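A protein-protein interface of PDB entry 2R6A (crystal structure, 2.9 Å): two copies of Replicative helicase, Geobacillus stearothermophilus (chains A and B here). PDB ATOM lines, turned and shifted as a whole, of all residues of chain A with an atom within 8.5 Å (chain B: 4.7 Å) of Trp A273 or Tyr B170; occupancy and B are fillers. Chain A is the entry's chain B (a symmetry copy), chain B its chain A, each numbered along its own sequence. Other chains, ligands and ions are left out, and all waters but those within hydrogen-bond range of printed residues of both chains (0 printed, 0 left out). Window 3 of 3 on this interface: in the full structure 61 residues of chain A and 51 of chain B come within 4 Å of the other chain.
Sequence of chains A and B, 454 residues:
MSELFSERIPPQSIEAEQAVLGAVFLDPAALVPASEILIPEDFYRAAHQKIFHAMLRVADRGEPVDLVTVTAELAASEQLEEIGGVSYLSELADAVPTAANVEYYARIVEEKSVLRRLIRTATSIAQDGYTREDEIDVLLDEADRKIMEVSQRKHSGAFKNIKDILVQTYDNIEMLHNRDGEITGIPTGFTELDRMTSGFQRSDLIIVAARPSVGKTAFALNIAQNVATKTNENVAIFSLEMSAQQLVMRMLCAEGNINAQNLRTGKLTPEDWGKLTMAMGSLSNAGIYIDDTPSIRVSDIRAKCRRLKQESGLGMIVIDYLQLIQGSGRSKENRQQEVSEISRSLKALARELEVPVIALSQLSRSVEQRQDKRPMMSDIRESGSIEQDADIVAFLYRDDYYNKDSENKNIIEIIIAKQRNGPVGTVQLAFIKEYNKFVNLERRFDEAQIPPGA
Among the printed residues, pairs that only touch across the chains: Leu A268 with His B177, Met A280 with Leu B166, Trp A273 with Ile B173, Val A248 with Leu B166, Trp A273 with His B177, Gln A245 with Thr B169, Met A280 with Tyr B170, Trp A273 with Tyr B170, Leu A252 with Leu B166, Leu A268 with Ile B173 and Lys A267 with His B177.
The backbone carbonyl oxygen (O) of Trp A273 lies within hydrogen-bond range of the side-chain hydroxyl (OG1) of Thr A277, 3.2 Å away.
No position is printed for both chains.
Of the 13 pairs that touch across the chains among the printed residues, none has its exchanged pair printed and touching as well.
Hydrophobic or aromatic side chains of chain B within 4 Å of the printed part of chain A: Leu B166, Tyr B170, Ile B173 and His B177.
Of the 22 printed residues of chain A, 8 touch a printed residue of chain B.
Printed residues of chain A that touch a printed residue of chain B: Gln A245, Val A248, Leu A252, Gly A266, Lys A267, Leu A268, Trp A273 and Met A280.
Hydrophobic or aromatic side chains of chain A that line the printed part of chain B: Val A248, Leu A252, Leu A268, Trp A273 and Met A280.
Among the printed residues, no Asp or Glu carboxylate lies within 4 Å of a Lys or Arg side-chain nitrogen of the other chain.
The side-chain amide oxygen (OE1) of Gln B168 lies close to the side-chain amide oxygen (OE1) of Gln A245, at 3.0 Å.
O of Gly A266 is in hydrogen-bond range of NE2 of His B177 (2.6 Å).
Printed residues of chain B within 4 Å of Gln A245: Gln B168 (3.0 Å) and Thr B169 (3.7 Å).
Of the printed residues of chain B, Lys A267 touches His B177 (3.8 Å).
Of chain B, only Tyr B170, Ile B173 and His B177 come within 4 Å of Trp A273.
Of chain A, only Trp A273 and Met A280 come within 4 Å of Tyr B170.
The nearest printed residue of chain B that does not touch Trp A273 is Glu B174 (4.8 Å).
The nearest residue of chain A that does not touch Tyr B170 is Leu A276 (4.4 Å).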
ATOM      1  N   GLN A 245       6.595 -17.362  -3.932  1.00  0.00           N
ATOM      2  CA  GLN A 245       6.939 -18.726  -4.340  1.00  0.00           C
ATOM      3  C   GLN A 245       5.770 -19.690  -4.190  1.00  0.00           C
ATOM      4  O   GLN A 245       5.479 -20.468  -5.096  1.00  0.00           O
ATOM      5  CB  GLN A 245       8.113 -19.241  -3.504  1.00  0.00           C
ATOM      6  CG  GLN A 245       9.488 -18.822  -3.991  1.00  0.00           C
ATOM      7  CD  GLN A 245      10.038 -19.736  -5.078  1.00  0.00           C
ATOM      8  OE1 GLN A 245      10.877 -19.320  -5.873  1.00  0.00           O
ATOM      9  NE2 GLN A 245       9.569 -20.986  -5.113  1.00  0.00           N
ATOM     10  N   VAL A 248       2.867 -18.734  -6.623  1.00  0.00           N
ATOM     11  CA  VAL A 248       3.080 -19.161  -8.013  1.00  0.00           C
ATOM     12  C   VAL A 248       2.930 -20.683  -8.142  1.00  0.00           C
ATOM     13  O   VAL A 248       2.445 -21.184  -9.157  1.00  0.00           O
ATOM     14  CB  VAL A 248       4.438 -18.675  -8.569  1.00  0.00           C
ATOM     15  CG1 VAL A 248       4.659 -19.188  -9.976  1.00  0.00           C
ATOM     16  CG2 VAL A 248       4.494 -17.161  -8.568  1.00  0.00           C
ATOM     17  N   MET A 249       3.344 -21.400  -7.099  1.00  0.00           N
ATOM     18  CA  MET A 249       3.179 -22.848  -7.006  1.00  0.00           C
ATOM     19  C   MET A 249       1.721 -23.264  -7.121  1.00  0.00           C
ATOM     20  O   MET A 249       1.407 -24.208  -7.838  1.00  0.00           O
ATOM     21  CB  MET A 249       3.751 -23.359  -5.685  1.00  0.00           C
ATOM     22  CG  MET A 249       5.135 -23.957  -5.793  1.00  0.00           C
ATOM     23  SD  MET A 249       5.041 -25.639  -6.442  1.00  0.00           S
ATOM     24  CE  MET A 249       4.024 -26.427  -5.177  1.00  0.00           C
ATOM     25  N   LEU A 252       0.355 -22.307 -11.035  1.00  0.00           N
ATOM     26  CA  LEU A 252       0.645 -23.272 -12.109  1.00  0.00           C
ATOM     27  C   LEU A 252       0.089 -24.656 -11.808  1.00  0.00           C
ATOM     28  O   LEU A 252      -0.121 -25.467 -12.710  1.00  0.00           O
ATOM     29  CB  LEU A 252       2.123 -23.291 -12.550  1.00  0.00           C
ATOM     30  CG  LEU A 252       3.331 -23.176 -11.624  1.00  0.00           C
ATOM     31  CD1 LEU A 252       3.494 -24.389 -10.724  1.00  0.00           C
ATOM     32  CD2 LEU A 252       4.561 -22.985 -12.495  1.00  0.00           C
ATOM     33  N   ILE A 258      -2.296 -29.771 -12.221  1.00  0.00           N
ATOM     34  CA  ILE A 258      -1.231 -30.597 -11.665  1.00  0.00           C
ATOM     35  C   ILE A 258      -1.485 -30.830 -10.180  1.00  0.00           C
ATOM     36  O   ILE A 258      -1.814 -29.904  -9.445  1.00  0.00           O
ATOM     37  CB  ILE A 258       0.166 -29.959 -11.861  1.00  0.00           C
ATOM     38  CG1 ILE A 258       0.320 -29.407 -13.281  1.00  0.00           C
ATOM     39  CG2 ILE A 258       1.251 -30.984 -11.576  1.00  0.00           C
ATOM     40  CD1 ILE A 258       1.461 -28.433 -13.438  1.00  0.00           C
ATOM     41  N   ASN A 262       2.528 -33.741  -5.785  1.00  0.00           N
ATOM     42  CA  ASN A 262       3.616 -34.205  -6.633  1.00  0.00           C
ATOM     43  C   ASN A 262       4.692 -33.150  -6.867  1.00  0.00           C
ATOM     44  O   ASN A 262       5.870 -33.481  -6.986  1.00  0.00           O
ATOM     45  CB  ASN A 262       3.052 -34.731  -7.947  1.00  0.00           C
ATOM     46  CG  ASN A 262       1.968 -35.767  -7.729  1.00  0.00           C
ATOM     47  OD1 ASN A 262       0.871 -35.653  -8.275  1.00  0.00           O
ATOM     48  ND2 ASN A 262       2.253 -36.765  -6.892  1.00  0.00           N
ATOM     49  N   LEU A 263       4.281 -31.885  -6.935  1.00  0.00           N
ATOM     50  CA  LEU A 263       5.214 -30.767  -7.048  1.00  0.00           C
ATOM     51  C   LEU A 263       6.021 -30.646  -5.754  1.00  0.00           C
ATOM     52  O   LEU A 263       7.240 -30.480  -5.783  1.00  0.00           O
ATOM     53  CB  LEU A 263       4.466 -29.459  -7.325  1.00  0.00           C
ATOM     54  CG  LEU A 263       4.095 -28.990  -8.739  1.00  0.00           C
ATOM     55  CD1 LEU A 263       3.415 -30.060  -9.542  1.00  0.00           C
ATOM     56  CD2 LEU A 263       3.207 -27.756  -8.685  1.00  0.00           C
ATOM     57  N   GLY A 266       8.832 -33.749  -4.587  1.00  0.00           N
ATOM     58  CA  GLY A 266       9.679 -33.981  -5.758  1.00  0.00           C
ATOM     59  C   GLY A 266       9.065 -34.737  -6.929  1.00  0.00           C
ATOM     60  O   GLY A 266       8.644 -34.131  -7.913  1.00  0.00           O
ATOM     61  N   LYS A 267       9.010 -36.063  -6.796  1.00  0.00           N
ATOM     62  CA  LYS A 267       8.545 -36.986  -7.841  1.00  0.00           C
ATOM     63  C   LYS A 267       7.326 -36.585  -8.709  1.00  0.00           C
ATOM     64  O   LYS A 267       6.178 -36.572  -8.250  1.00  0.00           O
ATOM     65  CB  LYS A 267       8.399 -38.409  -7.278  1.00  0.00           C
ATOM     66  CG  LYS A 267       9.729 -39.168  -7.190  1.00  0.00           C
ATOM     67  CD  LYS A 267       9.532 -40.689  -7.107  1.00  0.00           C
ATOM     68  CE  LYS A 267      10.869 -41.418  -7.177  1.00  0.00           C
ATOM     69  NZ  LYS A 267      10.734 -42.855  -6.850  1.00  0.00           N
ATOM     70  N   LEU A 268       7.625 -36.281  -9.975  1.00  0.00           N
ATOM     71  CA  LEU A 268       6.641 -35.900 -10.987  1.00  0.00           C
ATOM     72  C   LEU A 268       6.584 -36.946 -12.087  1.00  0.00           C
ATOM     73  O   LEU A 268       7.618 -37.401 -12.587  1.00  0.00           O
ATOM     74  CB  LEU A 268       7.015 -34.569 -11.644  1.00  0.00           C
ATOM     75  CG  LEU A 268       7.040 -33.242 -10.894  1.00  0.00           C
ATOM     76  CD1 LEU A 268       7.531 -32.186 -11.864  1.00  0.00           C
ATOM     77  CD2 LEU A 268       5.669 -32.879 -10.373  1.00  0.00           C
ATOM     78  N   THR A 269       5.389 -37.317 -12.492  1.00  0.00           N
ATOM     79  CA  THR A 269       5.246 -38.237 -13.560  1.00  0.00           C
ATOM     80  C   THR A 269       5.357 -37.455 -14.828  1.00  0.00           C
ATOM     81  O   THR A 269       5.302 -36.261 -14.783  1.00  0.00           O
ATOM     82  CB  THR A 269       3.945 -38.939 -13.464  1.00  0.00           C
ATOM     83  OG1 THR A 269       2.886 -38.003 -13.527  1.00  0.00           O
ATOM     84  CG2 THR A 269       3.870 -39.630 -12.207  1.00  0.00           C
ATOM     85  N   PRO A 270       5.559 -38.112 -15.954  1.00  0.00           N
ATOM     86  CA  PRO A 270       5.710 -37.386 -17.200  1.00  0.00           C
ATOM     87  C   PRO A 270       4.440 -36.755 -17.705  1.00  0.00           C
ATOM     88  O   PRO A 270       4.502 -35.955 -18.587  1.00  0.00           O
ATOM     89  CB  PRO A 270       6.219 -38.446 -18.190  1.00  0.00           C
ATOM     90  CG  PRO A 270       6.226 -39.690 -17.529  1.00  0.00           C
ATOM     91  CD  PRO A 270       5.687 -39.562 -16.153  1.00  0.00           C
ATOM     92  N   GLU A 271       3.293 -37.120 -17.179  1.00  0.00           N
ATOM     93  CA  GLU A 271       2.109 -36.328 -17.441  1.00  0.00           C
ATOM     94  C   GLU A 271       2.249 -34.979 -16.788  1.00  0.00           C
ATOM     95  O   GLU A 271       1.801 -33.994 -17.314  1.00  0.00           O
ATOM     96  CB  GLU A 271       0.806 -37.040 -17.030  1.00  0.00           C
ATOM     97  CG  GLU A 271      -0.405 -36.651 -17.858  1.00  0.00           C
ATOM     98  CD  GLU A 271      -1.695 -37.170 -17.308  1.00  0.00           C
ATOM     99  OE1 GLU A 271      -1.615 -37.996 -16.400  1.00  0.00           O
ATOM    100  OE2 GLU A 271      -2.783 -36.755 -17.777  1.00  0.00           O
ATOM    101  N   ASP A 272       2.933 -34.936 -15.656  1.00  0.00           N
ATOM    102  CA  ASP A 272       3.084 -33.735 -14.864  1.00  0.00           C
ATOM    103  C   ASP A 272       4.109 -32.839 -15.469  1.00  0.00           C
ATOM    104  O   ASP A 272       3.939 -31.659 -15.493  1.00  0.00           O
ATOM    105  CB  ASP A 272       3.527 -34.100 -13.467  1.00  0.00           C
ATOM    106  CG  ASP A 272       2.397 -34.583 -12.597  1.00  0.00           C
ATOM    107  OD1 ASP A 272       1.238 -34.266 -12.861  1.00  0.00           O
ATOM    108  OD2 ASP A 272       2.679 -35.275 -11.621  1.00  0.00           O
ATOM    109  N   TRP A 273       5.193 -33.405 -15.948  1.00  0.00           N
ATOM    110  CA  TRP A 273       6.237 -32.620 -16.608  1.00  0.00           C
ATOM    111  C   TRP A 273       5.731 -31.847 -17.818  1.00  0.00           C
ATOM    112  O   TRP A 273       5.943 -30.638 -17.918  1.00  0.00           O
ATOM    113  CB  TRP A 273       7.422 -33.501 -17.009  1.00  0.00           C
ATOM    114  CG  TRP A 273       8.348 -33.793 -15.889  1.00  0.00           C
ATOM    115  CD1 TRP A 273       8.502 -34.982 -15.238  1.00  0.00           C
ATOM    116  CD2 TRP A 273       9.251 -32.869 -15.262  1.00  0.00           C
ATOM    117  NE1 TRP A 273       9.451 -34.860 -14.245  1.00  0.00           N
ATOM    118  CE2 TRP A 273       9.925 -33.574 -14.238  1.00  0.00           C
ATOM    119  CE3 TRP A 273       9.557 -31.515 -15.468  1.00  0.00           C
ATOM    120  CZ2 TRP A 273      10.889 -32.972 -13.418  1.00  0.00           C
ATOM    121  CZ3 TRP A 273      10.515 -30.914 -14.650  1.00  0.00           C
ATOM    122  CH2 TRP A 273      11.170 -31.647 -13.640  1.00  0.00           C
ATOM    123  N   GLY A 274       5.070 -32.550 -18.735  1.00  0.00           N
ATOM    124  CA  GLY A 274       4.518 -31.930 -19.933  1.00  0.00           C
ATOM    125  C   GLY A 274       3.406 -30.981 -19.546  1.00  0.00           C
ATOM    126  O   GLY A 274       3.228 -29.925 -20.148  1.00  0.00           O
ATOM    127  N   LYS A 275       2.670 -31.365 -18.512  1.00  0.00           N
ATOM    128  CA  LYS A 275       1.570 -30.582 -17.984  1.00  0.00           C
ATOM    129  C   LYS A 275       2.099 -29.323 -17.289  1.00  0.00           C
ATOM    130  O   LYS A 275       1.392 -28.322 -17.190  1.00  0.00           O
ATOM    131  CB  LYS A 275       0.771 -31.445 -17.007  1.00  0.00           C
ATOM    132  CG  LYS A 275      -0.698 -31.122 -16.931  1.00  0.00           C
ATOM    133  CD  LYS A 275      -1.405 -31.957 -15.865  1.00  0.00           C
ATOM    134  CE  LYS A 275      -1.866 -33.311 -16.364  1.00  0.00           C
ATOM    135  NZ  LYS A 275      -2.587 -34.038 -15.283  1.00  0.00           N
ATOM    136  N   LEU A 276       3.346 -29.385 -16.821  1.00  0.00           N
ATOM    137  CA  LEU A 276       4.004 -28.269 -16.134  1.00  0.00           C
ATOM    138  C   LEU A 276       4.605 -27.265 -17.113  1.00  0.00           C
ATOM    139  O   LEU A 276       4.364 -26.058 -16.994  1.00  0.00           O
ATOM    140  CB  LEU A 276       5.089 -28.787 -15.175  1.00  0.00           C
ATOM    141  CG  LEU A 276       5.985 -27.781 -14.445  1.00  0.00           C
ATOM    142  CD1 LEU A 276       5.186 -26.938 -13.475  1.00  0.00           C
ATOM    143  CD2 LEU A 276       7.112 -28.493 -13.724  1.00  0.00           C
ATOM    144  N   THR A 277       5.395 -27.770 -18.068  1.00  0.00           N
ATOM    145  CA  THR A 277       6.025 -26.932 -19.097  1.00  0.00           C
ATOM    146  C   THR A 277       4.960 -26.134 -19.856  1.00  0.00           C
ATOM    147  O   THR A 277       5.221 -25.039 -20.366  1.00  0.00           O
ATOM    148  CB  THR A 277       6.914 -27.755 -20.088  1.00  0.00           C
ATOM    149  OG1 THR A 277       6.188 -28.887 -20.574  1.00  0.00           O
ATOM    150  CG2 THR A 277       8.190 -28.241 -19.407  1.00  0.00           C
ATOM    151  N   MET A 278       3.754 -26.694 -19.888  1.00  0.00           N
ATOM    152  CA  MET A 278       2.598 -26.071 -20.508  1.00  0.00           C
ATOM    153  C   MET A 278       2.092 -24.921 -19.650  1.00  0.00           C
ATOM    154  O   MET A 278       1.854 -23.820 -20.149  1.00  0.00           O
ATOM    155  CB  MET A 278       1.499 -27.118 -20.673  1.00  0.00           C
ATOM    156  CG  MET A 278       0.306 -26.680 -21.488  1.00  0.00           C
ATOM    157  SD  MET A 278      -0.352 -28.097 -22.397  1.00  0.00           S
ATOM    158  CE  MET A 278       0.950 -28.416 -23.613  1.00  0.00           C
ATOM    159  N   ALA A 279       1.951 -25.193 -18.356  1.00  0.00           N
ATOM    160  CA  ALA A 279       1.412 -24.239 -17.400  1.00  0.00           C
ATOM    161  C   ALA A 279       2.293 -23.011 -17.178  1.00  0.00           C
ATOM    162  O   ALA A 279       1.770 -21.925 -16.935  1.00  0.00           O
ATOM    163  CB  ALA A 279       1.103 -24.932 -16.068  1.00  0.00           C
ATOM    164  N   MET A 280       3.613 -23.164 -17.258  1.00  0.00           N
ATOM    165  CA  MET A 280       4.483 -22.011 -17.009  1.00  0.00           C
ATOM    166  C   MET A 280       4.886 -21.241 -18.245  1.00  0.00           C
ATOM    167  O   MET A 280       5.353 -20.105 -18.147  1.00  0.00           O
ATOM    168  CB  MET A 280       5.687 -22.350 -16.119  1.00  0.00           C
ATOM    169  CG  MET A 280       6.592 -23.473 -16.580  1.00  0.00           C
ATOM    170  SD  MET A 280       7.832 -23.758 -15.293  1.00  0.00           S
ATOM    171  CE  MET A 280       8.873 -22.307 -15.478  1.00  0.00           C
ATOM    172  N   LEU B 166       9.060 -18.034 -11.651  1.00  0.00           N
ATOM    173  CA  LEU B 166       8.925 -19.285 -12.401  1.00  0.00           C
ATOM    174  C   LEU B 166      10.282 -19.964 -12.553  1.00  0.00           C
ATOM    175  O   LEU B 166      10.384 -21.189 -12.461  1.00  0.00           O
ATOM    176  CB  LEU B 166       8.304 -19.048 -13.783  1.00  0.00           C
ATOM    177  CG  LEU B 166       6.848 -18.591 -13.918  1.00  0.00           C
ATOM    178  CD1 LEU B 166       6.527 -18.302 -15.378  1.00  0.00           C
ATOM    179  CD2 LEU B 166       5.874 -19.608 -13.346  1.00  0.00           C
ATOM    180  N   VAL B 167      11.311 -19.149 -12.783  1.00  0.00           N
ATOM    181  CA  VAL B 167      12.693 -19.616 -12.890  1.00  0.00           C
ATOM    182  C   VAL B 167      13.126 -20.253 -11.561  1.00  0.00           C
ATOM    183  O   VAL B 167      13.590 -21.394 -11.540  1.00  0.00           O
ATOM    184  CB  VAL B 167      13.653 -18.465 -13.320  1.00  0.00           C
ATOM    185  CG1 VAL B 167      15.113 -18.886 -13.210  1.00  0.00           C
ATOM    186  CG2 VAL B 167      13.329 -17.998 -14.742  1.00  0.00           C
ATOM    187  N   GLN B 168      12.947 -19.523 -10.461  1.00  0.00           N
ATOM    188  CA  GLN B 168      13.263 -20.039  -9.127  1.00  0.00           C
ATOM    189  C   GLN B 168      12.454 -21.299  -8.826  1.00  0.00           C
ATOM    190  O   GLN B 168      12.979 -22.254  -8.243  1.00  0.00           O
ATOM    191  CB  GLN B 168      12.993 -18.986  -8.054  1.00  0.00           C
ATOM    192  CG  GLN B 168      13.942 -17.795  -8.049  1.00  0.00           C
ATOM    193  CD  GLN B 168      13.511 -16.718  -7.060  1.00  0.00           C
ATOM    194  OE1 GLN B 168      12.418 -16.780  -6.492  1.00  0.00           O
ATOM    195  NE2 GLN B 168      14.367 -15.721  -6.856  1.00  0.00           N
ATOM    196  N   THR B 169      11.182 -21.287  -9.230  1.00  0.00           N
ATOM    197  CA  THR B 169      10.270 -22.421  -9.053  1.00  0.00           C
ATOM    198  C   THR B 169      10.768 -23.642  -9.814  1.00  0.00           C
ATOM    199  O   THR B 169      10.817 -24.743  -9.264  1.00  0.00           O
ATOM    200  CB  THR B 169       8.820 -22.072  -9.490  1.00  0.00           C
ATOM    201  OG1 THR B 169       8.248 -21.152  -8.552  1.00  0.00           O
ATOM    202  CG2 THR B 169       7.946 -23.310  -9.537  1.00  0.00           C
ATOM    203  N   TYR B 170      11.149 -23.438 -11.070  1.00  0.00           N
ATOM    204  CA  TYR B 170      11.626 -24.531 -11.903  1.00  0.00           C
ATOM    205  C   TYR B 170      12.963 -25.066 -11.393  1.00  0.00           C
ATOM    206  O   TYR B 170      13.172 -26.280 -11.364  1.00  0.00           O
ATOM    207  CB  TYR B 170      11.721 -24.108 -13.374  1.00  0.00           C
ATOM    208  CG  TYR B 170      11.861 -25.277 -14.317  1.00  0.00           C
ATOM    209  CD1 TYR B 170      10.738 -25.983 -14.749  1.00  0.00           C
ATOM    210  CD2 TYR B 170      13.117 -25.692 -14.763  1.00  0.00           C
ATOM    211  CE1 TYR B 170      10.862 -27.070 -15.602  1.00  0.00           C
ATOM    212  CE2 TYR B 170      13.255 -26.777 -15.619  1.00  0.00           C
ATOM    213  CZ  TYR B 170      12.126 -27.462 -16.037  1.00  0.00           C
ATOM    214  OH  TYR B 170      12.262 -28.534 -16.891  1.00  0.00           O
ATOM    215  N   ASP B 171      13.849 -24.158 -10.977  1.00  0.00           N
ATOM    216  CA  ASP B 171      15.164 -24.531 -10.437  1.00  0.00           C
ATOM    217  C   ASP B 171      15.038 -25.310  -9.136  1.00  0.00           C
ATOM    218  O   ASP B 171      15.927 -26.086  -8.778  1.00  0.00           O
ATOM    219  CB  ASP B 171      16.043 -23.301 -10.228  1.00  0.00           C
ATOM    220  CG  ASP B 171      16.469 -22.661 -11.532  1.00  0.00           C
ATOM    221  OD1 ASP B 171      16.683 -23.392 -12.529  1.00  0.00           O
ATOM    222  OD2 ASP B 171      16.598 -21.419 -11.557  1.00  0.00           O
ATOM    223  N   ASN B 172      13.935 -25.085  -8.429  1.00  0.00           N
ATOM    224  CA  ASN B 172      13.634 -25.831  -7.223  1.00  0.00           C
ATOM    225  C   ASN B 172      13.285 -27.263  -7.613  1.00  0.00           C
ATOM    226  O   ASN B 172      13.853 -28.217  -7.074  1.00  0.00           O
ATOM    227  CB  ASN B 172      12.478 -25.187  -6.462  1.00  0.00           C
ATOM    228  CG  ASN B 172      12.318 -25.748  -5.068  1.00  0.00           C
ATOM    229  OD1 ASN B 172      13.158 -25.523  -4.196  1.00  0.00           O
ATOM    230  ND2 ASN B 172      11.230 -26.473  -4.845  1.00  0.00           N
ATOM    231  N   ILE B 173      12.363 -27.396  -8.568  1.00  0.00           N
ATOM    232  CA  ILE B 173      11.951 -28.699  -9.100  1.00  0.00           C
ATOM    233  C   ILE B 173      13.167 -29.460  -9.643  1.00  0.00           C
ATOM    234  O   ILE B 173      13.217 -30.688  -9.573  1.00  0.00           O
ATOM    235  CB  ILE B 173      10.862 -28.569 -10.205  1.00  0.00           C
ATOM    236  CG1 ILE B 173       9.725 -27.620  -9.780  1.00  0.00           C
ATOM    237  CG2 ILE B 173      10.313 -29.935 -10.594  1.00  0.00           C
ATOM    238  CD1 ILE B 173       8.924 -28.046  -8.552  1.00  0.00           C
ATOM    239  N   GLU B 174      14.144 -28.725 -10.172  1.00  0.00           N
ATOM    240  CA  GLU B 174      15.399 -29.325 -10.625  1.00  0.00           C
ATOM    241  C   GLU B 174      16.112 -29.989  -9.448  1.00  0.00           C
ATOM    242  O   GLU B 174      16.444 -31.170  -9.520  1.00  0.00           O
ATOM    243  CB  GLU B 174      16.320 -28.290 -11.287  1.00  0.00           C
ATOM    244  CG  GLU B 174      15.776 -27.633 -12.565  1.00  0.00           C
ATOM    245  CD  GLU B 174      15.775 -28.540 -13.796  1.00  0.00           C
ATOM    246  OE1 GLU B 174      16.010 -28.012 -14.903  1.00  0.00           O
ATOM    247  OE2 GLU B 174      15.545 -29.764 -13.673  1.00  0.00           O
ATOM    248  N   HIS B 177      14.655 -33.266  -7.918  1.00  0.00           N
ATOM    249  CA  HIS B 177      14.848 -34.462  -8.756  1.00  0.00           C
ATOM    250  C   HIS B 177      16.328 -34.754  -8.966  1.00  0.00           C
ATOM    251  O   HIS B 177      16.733 -35.912  -9.075  1.00  0.00           O
ATOM    252  CB  HIS B 177      14.163 -34.286 -10.108  1.00  0.00           C
ATOM    253  CG  HIS B 177      12.669 -34.286 -10.029  1.00  0.00           C
ATOM    254  ND1 HIS B 177      11.894 -35.270 -10.615  1.00  0.00           N
ATOM    255  CD2 HIS B 177      11.808 -33.436  -9.413  1.00  0.00           C
ATOM    256  CE1 HIS B 177      10.620 -35.017 -10.377  1.00  0.00           C
ATOM    257  NE2 HIS B 177      10.540 -33.909  -9.651  1.00  0.00           N
